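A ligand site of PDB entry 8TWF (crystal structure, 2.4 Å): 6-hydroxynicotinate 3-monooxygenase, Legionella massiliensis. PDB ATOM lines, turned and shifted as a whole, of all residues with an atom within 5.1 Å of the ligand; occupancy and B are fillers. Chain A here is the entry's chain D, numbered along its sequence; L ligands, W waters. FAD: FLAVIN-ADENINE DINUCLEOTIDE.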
ATOM      1  N   ILE A  26     -22.336 -26.629   1.907  1.00  0.00           N
ATOM      2  CA  ILE A  26     -23.557 -25.922   1.527  1.00  0.00           C
ATOM      3  C   ILE A  26     -24.016 -25.079   2.705  1.00  0.00           C
ATOM      4  O   ILE A  26     -24.393 -25.620   3.758  1.00  0.00           O
ATOM      5  CB  ILE A  26     -24.670 -26.901   1.107  1.00  0.00           C
ATOM      6  CG1 ILE A  26     -24.191 -27.807  -0.031  1.00  0.00           C
ATOM      7  CG2 ILE A  26     -25.918 -26.133   0.699  1.00  0.00           C
ATOM      8  CD1 ILE A  26     -24.926 -29.142  -0.079  1.00  0.00           C
ATOM      9  N   GLY A  27     -24.028 -23.758   2.521  1.00  0.00           N
ATOM     10  CA  GLY A  27     -24.537 -22.856   3.537  1.00  0.00           C
ATOM     11  C   GLY A  27     -23.488 -21.934   4.146  1.00  0.00           C
ATOM     12  O   GLY A  27     -22.587 -22.388   4.845  1.00  0.00           O
ATOM     13  N   ALA A  28     -23.613 -20.628   3.886  1.00  0.00           N
ATOM     14  CA  ALA A  28     -22.643 -19.639   4.365  1.00  0.00           C
ATOM     15  C   ALA A  28     -23.171 -18.931   5.611  1.00  0.00           C
ATOM     16  O   ALA A  28     -23.382 -17.721   5.640  1.00  0.00           O
ATOM     17  CB  ALA A  28     -22.319 -18.646   3.260  1.00  0.00           C
ATOM     18  N   GLY A  29     -23.363 -19.717   6.674  1.00  0.00           N
ATOM     19  CA  GLY A  29     -23.805 -19.194   7.946  1.00  0.00           C
ATOM     20  C   GLY A  29     -22.707 -19.176   8.982  1.00  0.00           C
ATOM     21  O   GLY A  29     -21.770 -18.372   8.882  1.00  0.00           O
ATOM     22  N   ILE A  30     -22.792 -20.045   9.978  1.00  0.00           N
ATOM     23  CA  ILE A  30     -21.743 -20.226  10.975  1.00  0.00           C
ATOM     24  C   ILE A  30     -21.034 -21.567  10.792  1.00  0.00           C
ATOM     25  O   ILE A  30     -19.815 -21.610  10.641  1.00  0.00           O
ATOM     26  CB  ILE A  30     -22.293 -20.080  12.407  1.00  0.00           C
ATOM     27  CG1 ILE A  30     -22.750 -18.639  12.632  1.00  0.00           C
ATOM     28  CG2 ILE A  30     -21.258 -20.487  13.447  1.00  0.00           C
ATOM     29  CD1 ILE A  30     -23.662 -18.454  13.804  1.00  0.00           C
ATOM     30  N   ALA A  31     -21.794 -22.664  10.781  1.00  0.00           N
ATOM     31  CA  ALA A  31     -21.184 -23.985  10.645  1.00  0.00           C
ATOM     32  C   ALA A  31     -20.446 -24.123   9.321  1.00  0.00           C
ATOM     33  O   ALA A  31     -19.341 -24.689   9.282  1.00  0.00           O
ATOM     34  CB  ALA A  31     -22.260 -25.065  10.758  1.00  0.00           C
ATOM     35  N   GLY A  32     -21.026 -23.621   8.235  1.00  0.00           N
ATOM     36  CA  GLY A  32     -20.453 -23.767   6.920  1.00  0.00           C
ATOM     37  C   GLY A  32     -19.097 -23.106   6.801  1.00  0.00           C
ATOM     38  O   GLY A  32     -18.089 -23.743   6.503  1.00  0.00           O
ATOM     39  N   ILE A  49     -20.986 -22.741  -1.118  1.00  0.00           N
ATOM     40  CA  ILE A  49     -22.074 -22.127  -1.871  1.00  0.00           C
ATOM     41  C   ILE A  49     -23.111 -21.566  -0.911  1.00  0.00           C
ATOM     42  O   ILE A  49     -23.246 -22.008   0.236  1.00  0.00           O
ATOM     43  CB  ILE A  49     -22.764 -23.107  -2.854  1.00  0.00           C
ATOM     44  CG1 ILE A  49     -23.400 -24.284  -2.112  1.00  0.00           C
ATOM     45  CG2 ILE A  49     -21.780 -23.606  -3.902  1.00  0.00           C
ATOM     46  CD1 ILE A  49     -24.514 -24.967  -2.892  1.00  0.00           C
ATOM     47  N   GLU A  50     -23.855 -20.584  -1.395  1.00  0.00           N
ATOM     48  CA  GLU A  50     -24.901 -19.920  -0.634  1.00  0.00           C
ATOM     49  C   GLU A  50     -26.106 -19.704  -1.535  1.00  0.00           C
ATOM     50  O   GLU A  50     -25.965 -19.274  -2.680  1.00  0.00           O
ATOM     51  CB  GLU A  50     -24.415 -18.578  -0.061  1.00  0.00           C
ATOM     52  CG  GLU A  50     -25.514 -17.695   0.528  1.00  0.00           C
ATOM     53  CD  GLU A  50     -26.330 -18.379   1.624  1.00  0.00           C
ATOM     54  OE1 GLU A  50     -25.740 -19.154   2.422  1.00  0.00           O
ATOM     55  OE2 GLU A  50     -27.552 -18.142   1.685  1.00  0.00           O
ATOM     56  N   LYS A  51     -27.289 -20.006  -0.997  1.00  0.00           N
ATOM     57  CA  LYS A  51     -28.522 -19.855  -1.754  1.00  0.00           C
ATOM     58  C   LYS A  51     -28.811 -18.387  -2.062  1.00  0.00           C
ATOM     59  O   LYS A  51     -29.261 -18.066  -3.168  1.00  0.00           O
ATOM     60  CB  LYS A  51     -29.681 -20.477  -0.963  1.00  0.00           C
ATOM     61  CG  LYS A  51     -31.062 -20.327  -1.588  1.00  0.00           C
ATOM     62  CD  LYS A  51     -32.139 -20.863  -0.641  1.00  0.00           C
ATOM     63  CE  LYS A  51     -33.544 -20.483  -1.093  1.00  0.00           C
ATOM     64  NZ  LYS A  51     -34.537 -20.666   0.008  1.00  0.00           N
ATOM     65  N   TYR A  52     -28.558 -17.508  -1.107  1.00  0.00           N
ATOM     66  CA  TYR A  52     -28.874 -16.098  -1.278  1.00  0.00           C
ATOM     67  C   TYR A  52     -27.741 -15.363  -1.987  1.00  0.00           C
ATOM     68  O   TYR A  52     -26.579 -15.782  -1.955  1.00  0.00           O
ATOM     69  CB  TYR A  52     -29.161 -15.439   0.070  1.00  0.00           C
ATOM     70  CG  TYR A  52     -30.501 -15.847   0.662  1.00  0.00           C
ATOM     71  CD1 TYR A  52     -30.669 -17.098   1.246  1.00  0.00           C
ATOM     72  CD2 TYR A  52     -31.577 -14.980   0.652  1.00  0.00           C
ATOM     73  CE1 TYR A  52     -31.875 -17.480   1.785  1.00  0.00           C
ATOM     74  CE2 TYR A  52     -32.803 -15.348   1.188  1.00  0.00           C
ATOM     75  CZ  TYR A  52     -32.935 -16.601   1.761  1.00  0.00           C
ATOM     76  OH  TYR A  52     -34.148 -16.978   2.304  1.00  0.00           O
ATOM     77  N   ARG A  56     -25.844 -13.551   4.570  1.00  0.00           N
ATOM     78  CA  ARG A  56     -26.952 -13.198   5.452  1.00  0.00           C
ATOM     79  C   ARG A  56     -26.383 -12.829   6.815  1.00  0.00           C
ATOM     80  O   ARG A  56     -25.878 -13.683   7.547  1.00  0.00           O
ATOM     81  CB  ARG A  56     -27.936 -14.347   5.567  1.00  0.00           C
ATOM     82  CG  ARG A  56     -28.482 -14.812   4.226  1.00  0.00           C
ATOM     83  CD  ARG A  56     -29.375 -16.012   4.404  1.00  0.00           C
ATOM     84  NE  ARG A  56     -30.682 -15.657   4.941  1.00  0.00           N
ATOM     85  CZ  ARG A  56     -31.641 -16.522   5.232  1.00  0.00           C
ATOM     86  NH1 ARG A  56     -31.463 -17.823   5.077  1.00  0.00           N
ATOM     87  NH2 ARG A  56     -32.798 -16.070   5.692  1.00  0.00           N
ATOM     88  N   GLY A  58     -28.233 -11.173   9.208  1.00  0.00           N
ATOM     89  CA  GLY A  58     -29.288 -11.008  10.180  1.00  0.00           C
ATOM     90  C   GLY A  58     -29.034 -11.808  11.442  1.00  0.00           C
ATOM     91  O   GLY A  58     -28.071 -12.564  11.561  1.00  0.00           O
ATOM     92  N   GLY A  59     -29.929 -11.622  12.403  1.00  0.00           N
ATOM     93  CA  GLY A  59     -29.903 -12.360  13.650  1.00  0.00           C
ATOM     94  C   GLY A  59     -29.573 -11.468  14.845  1.00  0.00           C
ATOM     95  O   GLY A  59     -28.974 -10.387  14.715  1.00  0.00           O
ATOM     96  N   GLN A  60     -29.969 -11.941  16.020  1.00  0.00           N
ATOM     97  CA  GLN A  60     -29.723 -11.253  17.282  1.00  0.00           C
ATOM     98  C   GLN A  60     -28.310 -11.543  17.784  1.00  0.00           C
ATOM     99  O   GLN A  60     -27.513 -12.224  17.137  1.00  0.00           O
ATOM    100  CB  GLN A  60     -30.761 -11.662  18.320  1.00  0.00           C
ATOM    101  CG  GLN A  60     -32.065 -10.883  18.243  1.00  0.00           C
ATOM    102  CD  GLN A  60     -31.917  -9.428  18.690  1.00  0.00           C
ATOM    103  OE1 GLN A  60     -30.848  -9.007  19.155  1.00  0.00           O
ATOM    104  NE2 GLN A  60     -32.990  -8.645  18.553  1.00  0.00           N
ATOM    105  N   LEU A  62     -25.356 -13.247  19.804  1.00  0.00           N
ATOM    106  CA  LEU A  62     -25.001 -14.617  20.150  1.00  0.00           C
ATOM    107  C   LEU A  62     -23.864 -14.586  21.161  1.00  0.00           C
ATOM    108  O   LEU A  62     -23.172 -13.586  21.321  1.00  0.00           O
ATOM    109  CB  LEU A  62     -24.555 -15.414  18.917  1.00  0.00           C
ATOM    110  CG  LEU A  62     -25.526 -15.486  17.747  1.00  0.00           C
ATOM    111  CD1 LEU A  62     -24.918 -16.316  16.634  1.00  0.00           C
ATOM    112  CD2 LEU A  62     -26.864 -16.060  18.186  1.00  0.00           C
ATOM    113  N   ARG A 121     -24.805 -11.737  15.568  1.00  0.00           N
ATOM    114  CA  ARG A 121     -24.568 -12.862  14.671  1.00  0.00           C
ATOM    115  C   ARG A 121     -23.933 -12.402  13.363  1.00  0.00           C
ATOM    116  O   ARG A 121     -22.971 -13.014  12.884  1.00  0.00           O
ATOM    117  CB  ARG A 121     -25.880 -13.598  14.394  1.00  0.00           C
ATOM    118  CG  ARG A 121     -25.710 -14.772  13.421  1.00  0.00           C
ATOM    119  CD  ARG A 121     -27.026 -15.407  13.016  1.00  0.00           C
ATOM    120  NE  ARG A 121     -26.819 -16.452  12.023  1.00  0.00           N
ATOM    121  CZ  ARG A 121     -26.620 -16.250  10.730  1.00  0.00           C
ATOM    122  NH1 ARG A 121     -26.608 -15.021  10.228  1.00  0.00           N
ATOM    123  NH2 ARG A 121     -26.419 -17.280   9.922  1.00  0.00           N
ATOM    124  N   GLN A 141     -26.296 -19.778  -5.484  1.00  0.00           N
ATOM    125  CA  GLN A 141     -26.161 -21.174  -5.900  1.00  0.00           C
ATOM    126  C   GLN A 141     -26.965 -22.059  -4.946  1.00  0.00           C
ATOM    127  O   GLN A 141     -26.924 -21.873  -3.724  1.00  0.00           O
ATOM    128  CB  GLN A 141     -24.704 -21.633  -5.889  1.00  0.00           C
ATOM    129  CG  GLN A 141     -23.881 -21.094  -7.031  1.00  0.00           C
ATOM    130  CD  GLN A 141     -24.446 -21.483  -8.384  1.00  0.00           C
ATOM    131  OE1 GLN A 141     -24.768 -22.642  -8.633  1.00  0.00           O
ATOM    132  NE2 GLN A 141     -24.580 -20.494  -9.265  1.00  0.00           N
ATOM    133  N   SER A 142     -27.691 -23.015  -5.525  1.00  0.00           N
ATOM    134  CA  SER A 142     -28.507 -23.933  -4.736  1.00  0.00           C
ATOM    135  C   SER A 142     -28.699 -25.216  -5.518  1.00  0.00           C
ATOM    136  O   SER A 142     -28.669 -25.224  -6.751  1.00  0.00           O
ATOM    137  CB  SER A 142     -29.860 -23.303  -4.386  1.00  0.00           C
ATOM    138  OG  SER A 142     -30.599 -24.163  -3.541  1.00  0.00           O
ATOM    139  N   ILE A 143     -28.905 -26.308  -4.780  1.00  0.00           N
ATOM    140  CA  ILE A 143     -29.049 -27.648  -5.340  1.00  0.00           C
ATOM    141  C   ILE A 143     -30.531 -27.931  -5.602  1.00  0.00           C
ATOM    142  O   ILE A 143     -31.393 -27.521  -4.824  1.00  0.00           O
ATOM    143  CB  ILE A 143     -28.455 -28.696  -4.374  1.00  0.00           C
ATOM    144  CG1 ILE A 143     -26.951 -28.444  -4.211  1.00  0.00           C
ATOM    145  CG2 ILE A 143     -28.719 -30.120  -4.852  1.00  0.00           C
ATOM    146  CD1 ILE A 143     -26.284 -29.320  -3.160  1.00  0.00           C
ATOM    147  N   ALA A 171     -24.551 -27.494   5.616  1.00  0.00           N
ATOM    148  CA  ALA A 171     -24.651 -26.532   6.713  1.00  0.00           C
ATOM    149  C   ALA A 171     -25.707 -25.497   6.376  1.00  0.00           C
ATOM    150  O   ALA A 171     -25.497 -24.285   6.532  1.00  0.00           O
ATOM    151  CB  ALA A 171     -23.312 -25.871   6.991  1.00  0.00           C
ATOM    152  N   ASP A 172     -26.857 -25.950   5.880  1.00  0.00           N
ATOM    153  CA  ASP A 172     -27.872 -25.065   5.341  1.00  0.00           C
ATOM    154  C   ASP A 172     -29.053 -24.878   6.301  1.00  0.00           C
ATOM    155  O   ASP A 172     -30.114 -24.415   5.872  1.00  0.00           O
ATOM    156  CB  ASP A 172     -28.348 -25.560   3.966  1.00  0.00           C
ATOM    157  CG  ASP A 172     -28.675 -27.059   3.932  1.00  0.00           C
ATOM    158  OD1 ASP A 172     -28.400 -27.771   4.928  1.00  0.00           O
ATOM    159  OD2 ASP A 172     -29.203 -27.509   2.893  1.00  0.00           O
ATOM    160  N   GLY A 173     -28.880 -25.194   7.581  1.00  0.00           N
ATOM    161  CA  GLY A 173     -29.774 -24.721   8.617  1.00  0.00           C
ATOM    162  C   GLY A 173     -30.885 -25.702   8.982  1.00  0.00           C
ATOM    163  O   GLY A 173     -30.989 -26.809   8.449  1.00  0.00           O
ATOM    164  N   ILE A 174     -31.725 -25.232   9.909  1.00  0.00           N
ATOM    165  CA  ILE A 174     -32.779 -26.071  10.498  1.00  0.00           C
ATOM    166  C   ILE A 174     -33.621 -26.728   9.416  1.00  0.00           C
ATOM    167  O   ILE A 174     -33.952 -27.911   9.499  1.00  0.00           O
ATOM    168  CB  ILE A 174     -33.636 -25.235  11.463  1.00  0.00           C
ATOM    169  CG1 ILE A 174     -34.762 -26.066  12.090  1.00  0.00           C
ATOM    170  CG2 ILE A 174     -34.259 -24.039  10.741  1.00  0.00           C
ATOM    171  CD1 ILE A 174     -34.290 -27.038  13.128  1.00  0.00           C
ATOM    172  N   ALA A 177     -32.464 -28.165   3.090  1.00  0.00           N
ATOM    173  CA  ALA A 177     -32.931 -28.780   1.852  1.00  0.00           C
ATOM    174  C   ALA A 177     -32.095 -30.009   1.501  1.00  0.00           C
ATOM    175  O   ALA A 177     -32.597 -30.917   0.821  1.00  0.00           O
ATOM    176  CB  ALA A 177     -32.873 -27.769   0.708  1.00  0.00           C
ATOM    177  N   LEU A 197     -39.720 -17.123  17.114  1.00  0.00           N
ATOM    178  CA  LEU A 197     -38.777 -16.012  17.198  1.00  0.00           C
ATOM    179  C   LEU A 197     -38.728 -15.272  15.865  1.00  0.00           C
ATOM    180  O   LEU A 197     -38.818 -15.889  14.800  1.00  0.00           O
ATOM    181  CB  LEU A 197     -37.376 -16.515  17.583  1.00  0.00           C
ATOM    182  CG  LEU A 197     -36.190 -15.572  17.349  1.00  0.00           C
ATOM    183  CD1 LEU A 197     -36.313 -14.294  18.176  1.00  0.00           C
ATOM    184  CD2 LEU A 197     -34.891 -16.299  17.693  1.00  0.00           C
ATOM    185  N   THR A 199     -36.638 -11.579  14.160  1.00  0.00           N
ATOM    186  CA  THR A 199     -35.778 -10.417  14.339  1.00  0.00           C
ATOM    187  C   THR A 199     -35.453  -9.820  12.977  1.00  0.00           C
ATOM    188  O   THR A 199     -35.315 -10.535  11.993  1.00  0.00           O
ATOM    189  CB  THR A 199     -34.491 -10.781  15.091  1.00  0.00           C
ATOM    190  OG1 THR A 199     -33.658  -9.614  15.227  1.00  0.00           O
ATOM    191  CG2 THR A 199     -33.706 -11.851  14.349  1.00  0.00           C
ATOM    192  N   TYR A 283     -35.895 -12.334   9.543  1.00  0.00           N
ATOM    193  CA  TYR A 283     -35.745 -13.694  10.053  1.00  0.00           C
ATOM    194  C   TYR A 283     -36.961 -14.052  10.886  1.00  0.00           C
ATOM    195  O   TYR A 283     -37.348 -13.303  11.795  1.00  0.00           O
ATOM    196  CB  TYR A 283     -34.471 -13.839  10.879  1.00  0.00           C
ATOM    197  CG  TYR A 283     -34.326 -15.180  11.550  1.00  0.00           C
ATOM    198  CD1 TYR A 283     -33.801 -16.268  10.864  1.00  0.00           C
ATOM    199  CD2 TYR A 283     -34.708 -15.357  12.870  1.00  0.00           C
ATOM    200  CE1 TYR A 283     -33.668 -17.492  11.480  1.00  0.00           C
ATOM    201  CE2 TYR A 283     -34.583 -16.582  13.497  1.00  0.00           C
ATOM    202  CZ  TYR A 283     -34.055 -17.648  12.790  1.00  0.00           C
ATOM    203  OH  TYR A 283     -33.929 -18.867  13.411  1.00  0.00           O
ATOM    204  N   ILE A 303     -23.975 -30.975   9.355  1.00  0.00           N
ATOM    205  CA  ILE A 303     -23.366 -30.230  10.446  1.00  0.00           C
ATOM    206  C   ILE A 303     -24.268 -29.071  10.830  1.00  0.00           C
ATOM    207  O   ILE A 303     -25.075 -28.578  10.027  1.00  0.00           O
ATOM    208  CB  ILE A 303     -21.952 -29.709  10.094  1.00  0.00           C
ATOM    209  CG1 ILE A 303     -22.003 -28.718   8.928  1.00  0.00           C
ATOM    210  CG2 ILE A 303     -21.058 -30.867   9.739  1.00  0.00           C
ATOM    211  CD1 ILE A 303     -20.718 -27.949   8.748  1.00  0.00           C
ATOM    212  N   GLY A 304     -24.134 -28.622  12.076  1.00  0.00           N
ATOM    213  CA  GLY A 304     -24.884 -27.476  12.542  1.00  0.00           C
ATOM    214  C   GLY A 304     -26.371 -27.769  12.725  1.00  0.00           C
ATOM    215  O   GLY A 304     -26.790 -28.892  13.013  1.00  0.00           O
ATOM    216  N   ASP A 305     -27.176 -26.713  12.549  1.00  0.00           N
ATOM    217  CA  ASP A 305     -28.621 -26.826  12.722  1.00  0.00           C
ATOM    218  C   ASP A 305     -29.253 -27.837  11.774  1.00  0.00           C
ATOM    219  O   ASP A 305     -30.312 -28.389  12.092  1.00  0.00           O
ATOM    220  CB  ASP A 305     -29.290 -25.453  12.543  1.00  0.00           C
ATOM    221  CG  ASP A 305     -29.230 -24.590  13.795  1.00  0.00           C
ATOM    222  OD1 ASP A 305     -28.506 -24.943  14.754  1.00  0.00           O
ATOM    223  OD2 ASP A 305     -29.924 -23.552  13.817  1.00  0.00           O
ATOM    224  N   ALA A 306     -28.636 -28.099  10.620  1.00  0.00           N
ATOM    225  CA  ALA A 306     -29.167 -29.102   9.696  1.00  0.00           C
ATOM    226  C   ALA A 306     -29.253 -30.485  10.345  1.00  0.00           C
ATOM    227  O   ALA A 306     -30.099 -31.294   9.968  1.00  0.00           O
ATOM    228  CB  ALA A 306     -28.322 -29.161   8.426  1.00  0.00           C
ATOM    229  N   PRO A 312     -32.993 -21.693  19.497  1.00  0.00           N
ATOM    230  CA  PRO A 312     -32.489 -20.475  20.161  1.00  0.00           C
ATOM    231  C   PRO A 312     -32.587 -20.517  21.676  1.00  0.00           C
ATOM    232  O   PRO A 312     -31.753 -19.896  22.348  1.00  0.00           O
ATOM    233  CB  PRO A 312     -33.378 -19.374  19.560  1.00  0.00           C
ATOM    234  CG  PRO A 312     -33.863 -19.923  18.258  1.00  0.00           C
ATOM    235  CD  PRO A 312     -34.013 -21.400  18.488  1.00  0.00           C
ATOM    236  N   GLY A 317     -26.625 -22.785  19.586  1.00  0.00           N
ATOM    237  CA  GLY A 317     -26.567 -23.230  18.203  1.00  0.00           C
ATOM    238  C   GLY A 317     -25.242 -22.910  17.549  1.00  0.00           C
ATOM    239  O   GLY A 317     -24.629 -23.762  16.914  1.00  0.00           O
ATOM    240  N   ASN A 318     -24.793 -21.664  17.704  1.00  0.00           N
ATOM    241  CA  ASN A 318     -23.525 -21.268  17.089  1.00  0.00           C
ATOM    242  C   ASN A 318     -22.356 -22.048  17.672  1.00  0.00           C
ATOM    243  O   ASN A 318     -21.446 -22.451  16.953  1.00  0.00           O
ATOM    244  CB  ASN A 318     -23.309 -19.764  17.254  1.00  0.00           C
ATOM    245  CG  ASN A 318     -23.392 -19.325  18.713  1.00  0.00           C
ATOM    246  OD1 ASN A 318     -24.473 -19.225  19.286  1.00  0.00           O
ATOM    247  ND2 ASN A 318     -22.231 -19.044  19.308  1.00  0.00           N
ATOM    248  N   ALA A 321     -22.448 -25.502  16.375  1.00  0.00           N
ATOM    249  CA  ALA A 321     -21.941 -25.437  15.006  1.00  0.00           C
ATOM    250  C   ALA A 321     -20.415 -25.371  14.984  1.00  0.00           C
ATOM    251  O   ALA A 321     -19.771 -25.978  14.116  1.00  0.00           O
ATOM    252  CB  ALA A 321     -22.535 -24.237  14.279  1.00  0.00           C
HETATM  253  PA  FAD L   1     -27.580 -21.150   9.880  1.00  0.00           P
HETATM  254  O1A FAD L   1     -27.048 -20.089  10.776  1.00  0.00           O
HETATM  255  O2A FAD L   1     -29.115 -21.152   9.792  1.00  0.00           O
HETATM  256  O5B FAD L   1     -26.903 -21.054   8.440  1.00  0.00           O
HETATM  257  C5B FAD L   1     -27.513 -21.649   7.271  1.00  0.00           C
HETATM  258  C4B FAD L   1     -26.958 -20.996   6.017  1.00  0.00           C
HETATM  259  O4B FAD L   1     -27.234 -21.839   4.880  1.00  0.00           O
HETATM  260  C3B FAD L   1     -27.571 -19.632   5.695  1.00  0.00           C
HETATM  261  O3B FAD L   1     -26.565 -18.745   5.191  1.00  0.00           O
HETATM  262  C2B FAD L   1     -28.612 -19.968   4.620  1.00  0.00           C
HETATM  263  O2B FAD L   1     -28.883 -18.863   3.763  1.00  0.00           O
HETATM  264  C1B FAD L   1     -27.881 -21.079   3.873  1.00  0.00           C
HETATM  265  N9A FAD L   1     -28.747 -21.959   3.091  1.00  0.00           N
HETATM  266  C8A FAD L   1     -29.995 -22.411   3.424  1.00  0.00           C
HETATM  267  N7A FAD L   1     -30.531 -23.193   2.522  1.00  0.00           N
HETATM  268  C5A FAD L   1     -29.577 -23.259   1.519  1.00  0.00           C
HETATM  269  C6A FAD L   1     -29.537 -23.929   0.279  1.00  0.00           C
HETATM  270  N6A FAD L   1     -30.531 -24.690  -0.174  1.00  0.00           N
HETATM  271  N1A FAD L   1     -28.426 -23.774  -0.476  1.00  0.00           N
HETATM  272  C2A FAD L   1     -27.432 -23.013  -0.023  1.00  0.00           C
HETATM  273  N3A FAD L   1     -27.360 -22.334   1.131  1.00  0.00           N
HETATM  274  C4A FAD L   1     -28.472 -22.501   1.859  1.00  0.00           C
HETATM  275  N1  FAD L   1     -30.478 -18.202  15.640  1.00  0.00           N
HETATM  276  C2  FAD L   1     -30.876 -17.637  16.819  1.00  0.00           C
HETATM  277  O2  FAD L   1     -30.843 -18.264  17.878  1.00  0.00           O
HETATM  278  N3  FAD L   1     -31.325 -16.329  16.838  1.00  0.00           N
HETATM  279  C4  FAD L   1     -31.425 -15.488  15.742  1.00  0.00           C
HETATM  280  O4  FAD L   1     -31.841 -14.340  15.876  1.00  0.00           O
HETATM  281  C4X FAD L   1     -31.008 -16.103  14.502  1.00  0.00           C
HETATM  282  N5  FAD L   1     -31.073 -15.384  13.416  1.00  0.00           N
HETATM  283  C5X FAD L   1     -30.668 -15.965  12.222  1.00  0.00           C
HETATM  284  C6  FAD L   1     -30.731 -15.207  11.047  1.00  0.00           C
HETATM  285  C7  FAD L   1     -30.349 -15.740   9.827  1.00  0.00           C
HETATM  286  C7M FAD L   1     -30.434 -14.885   8.589  1.00  0.00           C
HETATM  287  C8  FAD L   1     -29.885 -17.064   9.764  1.00  0.00           C
HETATM  288  C8M FAD L   1     -29.459 -17.679   8.454  1.00  0.00           C
HETATM  289  C9  FAD L   1     -29.815 -17.821  10.927  1.00  0.00           C
HETATM  290  C9A FAD L   1     -30.211 -17.287  12.147  1.00  0.00           C
HETATM  291  N10 FAD L   1     -30.170 -18.032  13.360  1.00  0.00           N
HETATM  292  C10 FAD L   1     -30.546 -17.464  14.545  1.00  0.00           C
HETATM  293  C1' FAD L   1     -29.687 -19.413  13.372  1.00  0.00           C
HETATM  294  C2' FAD L   1     -28.279 -19.540  13.923  1.00  0.00           C
HETATM  295  O2' FAD L   1     -27.356 -18.984  12.986  1.00  0.00           O
HETATM  296  C3' FAD L   1     -27.945 -21.017  14.158  1.00  0.00           C
HETATM  297  O3' FAD L   1     -28.757 -21.496  15.219  1.00  0.00           O
HETATM  298  C4' FAD L   1     -26.477 -21.252  14.524  1.00  0.00           C
HETATM  299  O4' FAD L   1     -25.979 -20.079  15.172  1.00  0.00           O
HETATM  300  C5' FAD L   1     -25.607 -21.553  13.329  1.00  0.00           C
HETATM  301  O5' FAD L   1     -26.118 -22.721  12.656  1.00  0.00           O
HETATM  302  P   FAD L   1     -25.815 -22.996  11.140  1.00  0.00           P
HETATM  303  O1P FAD L   1     -24.676 -22.167  10.555  1.00  0.00           O
HETATM  304  O2P FAD L   1     -25.637 -24.466  11.042  1.00  0.00           O
HETATM  305  O3P FAD L   1     -27.162 -22.584  10.414  1.00  0.00           O
HETATM  306  O   HOH W   1     -25.978 -16.492   7.185  1.00  0.00           O
HETATM  307  O   HOH W   2     -28.315 -18.560  20.123  1.00  0.00           O
HETATM  308  O   HOH W   3     -26.609 -26.394   9.273  1.00  0.00           O
HETATM  309  O   HOH W   4     -32.595 -25.135   3.282  1.00  0.00           O
HETATM  310  O   HOH W   5     -27.211 -19.699  17.890  1.00  0.00           O
HETATM  311  O   HOH W   6     -31.684 -26.297  -2.206  1.00  0.00           O
HETATM  312  O   HOH W   7     -30.286 -20.799  17.538  1.00  0.00           O
HETATM  313  O   HOH W   8     -25.004 -16.369   4.190  1.00  0.00           O
HETATM  314  O   HOH W   9     -32.016 -15.283  19.658  1.00  0.00           O
HETATM  315  O   HOH W  10     -23.688 -22.364   7.883  1.00  0.00           O
HETATM  316  O   HOH W  11     -30.999 -22.785  11.335  1.00  0.00           O
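N of Ile 30 lies within hydrogen-bond range of O1P of the ligand (2.9 Å). The side-chain carboxylate (OE2) of Glu 50 lies within hydrogen-bond range of an oxygen (O2B) of the ligand (2.6 Å). The backbone NH (N) of Gln 60 lies within hydrogen-bond range of an oxygen (O4) of the ligand, at 3.0 Å. The guanidinium group (NH1) of Arg 56 lies close to an oxygen (O2B) of the ligand, at 3.1 Å. OG of Ser 142 sits at hydrogen-bond distance from N6A of the ligand (3.4 Å). The backbone carbonyl oxygen (O) of Ala 28 lies within hydrogen-bond range of an oxygen (O3B) of the ligand. N of Asn 318 sits at hydrogen-bond distance from O4' of the ligand (3.2 Å). The backbone NH (N) of Lys 51 sits at hydrogen-bond distance from a nitrogen (N3A) of the ligand, 3.2 Å away. The backbone NH of Ala 31 lies within hydrogen-bond range of an oxygen (O1P) of the ligand (2.9 Å). An oxygen (O2P) of the ligand is in hydrogen-bond range of the backbone NH (N) of Asp 305 (3.1 Å). OD2 of Asp 305 sits at hydrogen-bond distance from O3' of the ligand (2.7 Å). NH2 of Arg 121 is in salt-bridge range of O1A of the ligand (3.0 Å).
The backbone carbonyl oxygen (O) of Gln 60 is in hydrogen-bond range of the backbone NH (N) of Arg 121 (3.2 Å). The backbone carbonyl oxygen of Tyr 283 is in hydrogen-bond range of the backbone NH of Thr 199, 3.0 Å away. N of Ala 177 sits at hydrogen-bond distance from OD2 of Asp 172, at 3.3 Å. OE1 of Glu 50 sits at hydrogen-bond distance from N of Ala 28, at 3.0 Å. N of Ala 306 lies close to O of Gly 173 (3.5 Å). The backbone NH (N) of Gly 27 is in hydrogen-bond range of the backbone carbonyl oxygen (O) of Ile 49, at 3.0 Å. The backbone NH (N) of Asp 172 is in hydrogen-bond range of the backbone carbonyl oxygen (O) of Ile 26 (3.3 Å). N of Lys 51 lies close to O of Gln 141 (3.3 Å).
An oxygen (O4B) of the ligand lies close to the backbone carbonyl oxygen (O) of Ala 171, 3.4 Å away. Merely in contact with the ligand: Ile 26, Gly 27, Gly 29, Tyr 52, Gly 58, Gly 59, Gln 141, Asp 172, Gly 173, Ala 177, Leu 197, Thr 199, Tyr 283, Gly 304, Pro 312 and Gly 317. Hydrophobic or aromatic side chains that line the ligand: Ile 26, Ile 30, Ala 31, Tyr 52, Ala 177, Leu 197, Tyr 283 and Pro 312. Of the 36 residues printed, 28 come within 4 Å of the ligand.
Water W6 lies within hydrogen-bond range of the side-chain hydroxyl (OG) of Ser 142, a nitrogen (N6A) of the ligand and the backbone carbonyl oxygen (O) of Ile 143. Water W11 lies within hydrogen-bond range of OD2 of Asp 305 (2.8 Å), N of Ile 174 (2.9 Å) and O2A of the ligand (2.9 Å). Water W4 bridges a nitrogen (N7A) of the ligand and the backbone NH (N) of Ala 177. Water W5 lies within hydrogen-bond range of an oxygen (O4') of the ligand (3.0 Å) and the side-chain amide oxygen (OD1) of Asn 318 (3.1 Å). Water W8 lies within hydrogen-bond range of the backbone carbonyl oxygen of Ala 28 (2.6 Å), the backbone NH of Arg 56 (3.0 Å), an oxygen (O3B) of the ligand (3.0 Å) and the side-chain carboxylate of Glu 50 (3.4 Å). Water W1 lies within hydrogen-bond range of O of Arg 56 (2.8 Å), NH2 of Arg 121 (2.9 Å), O3B of the ligand (3.1 Å) and O of Ala 28 (3.3 Å).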
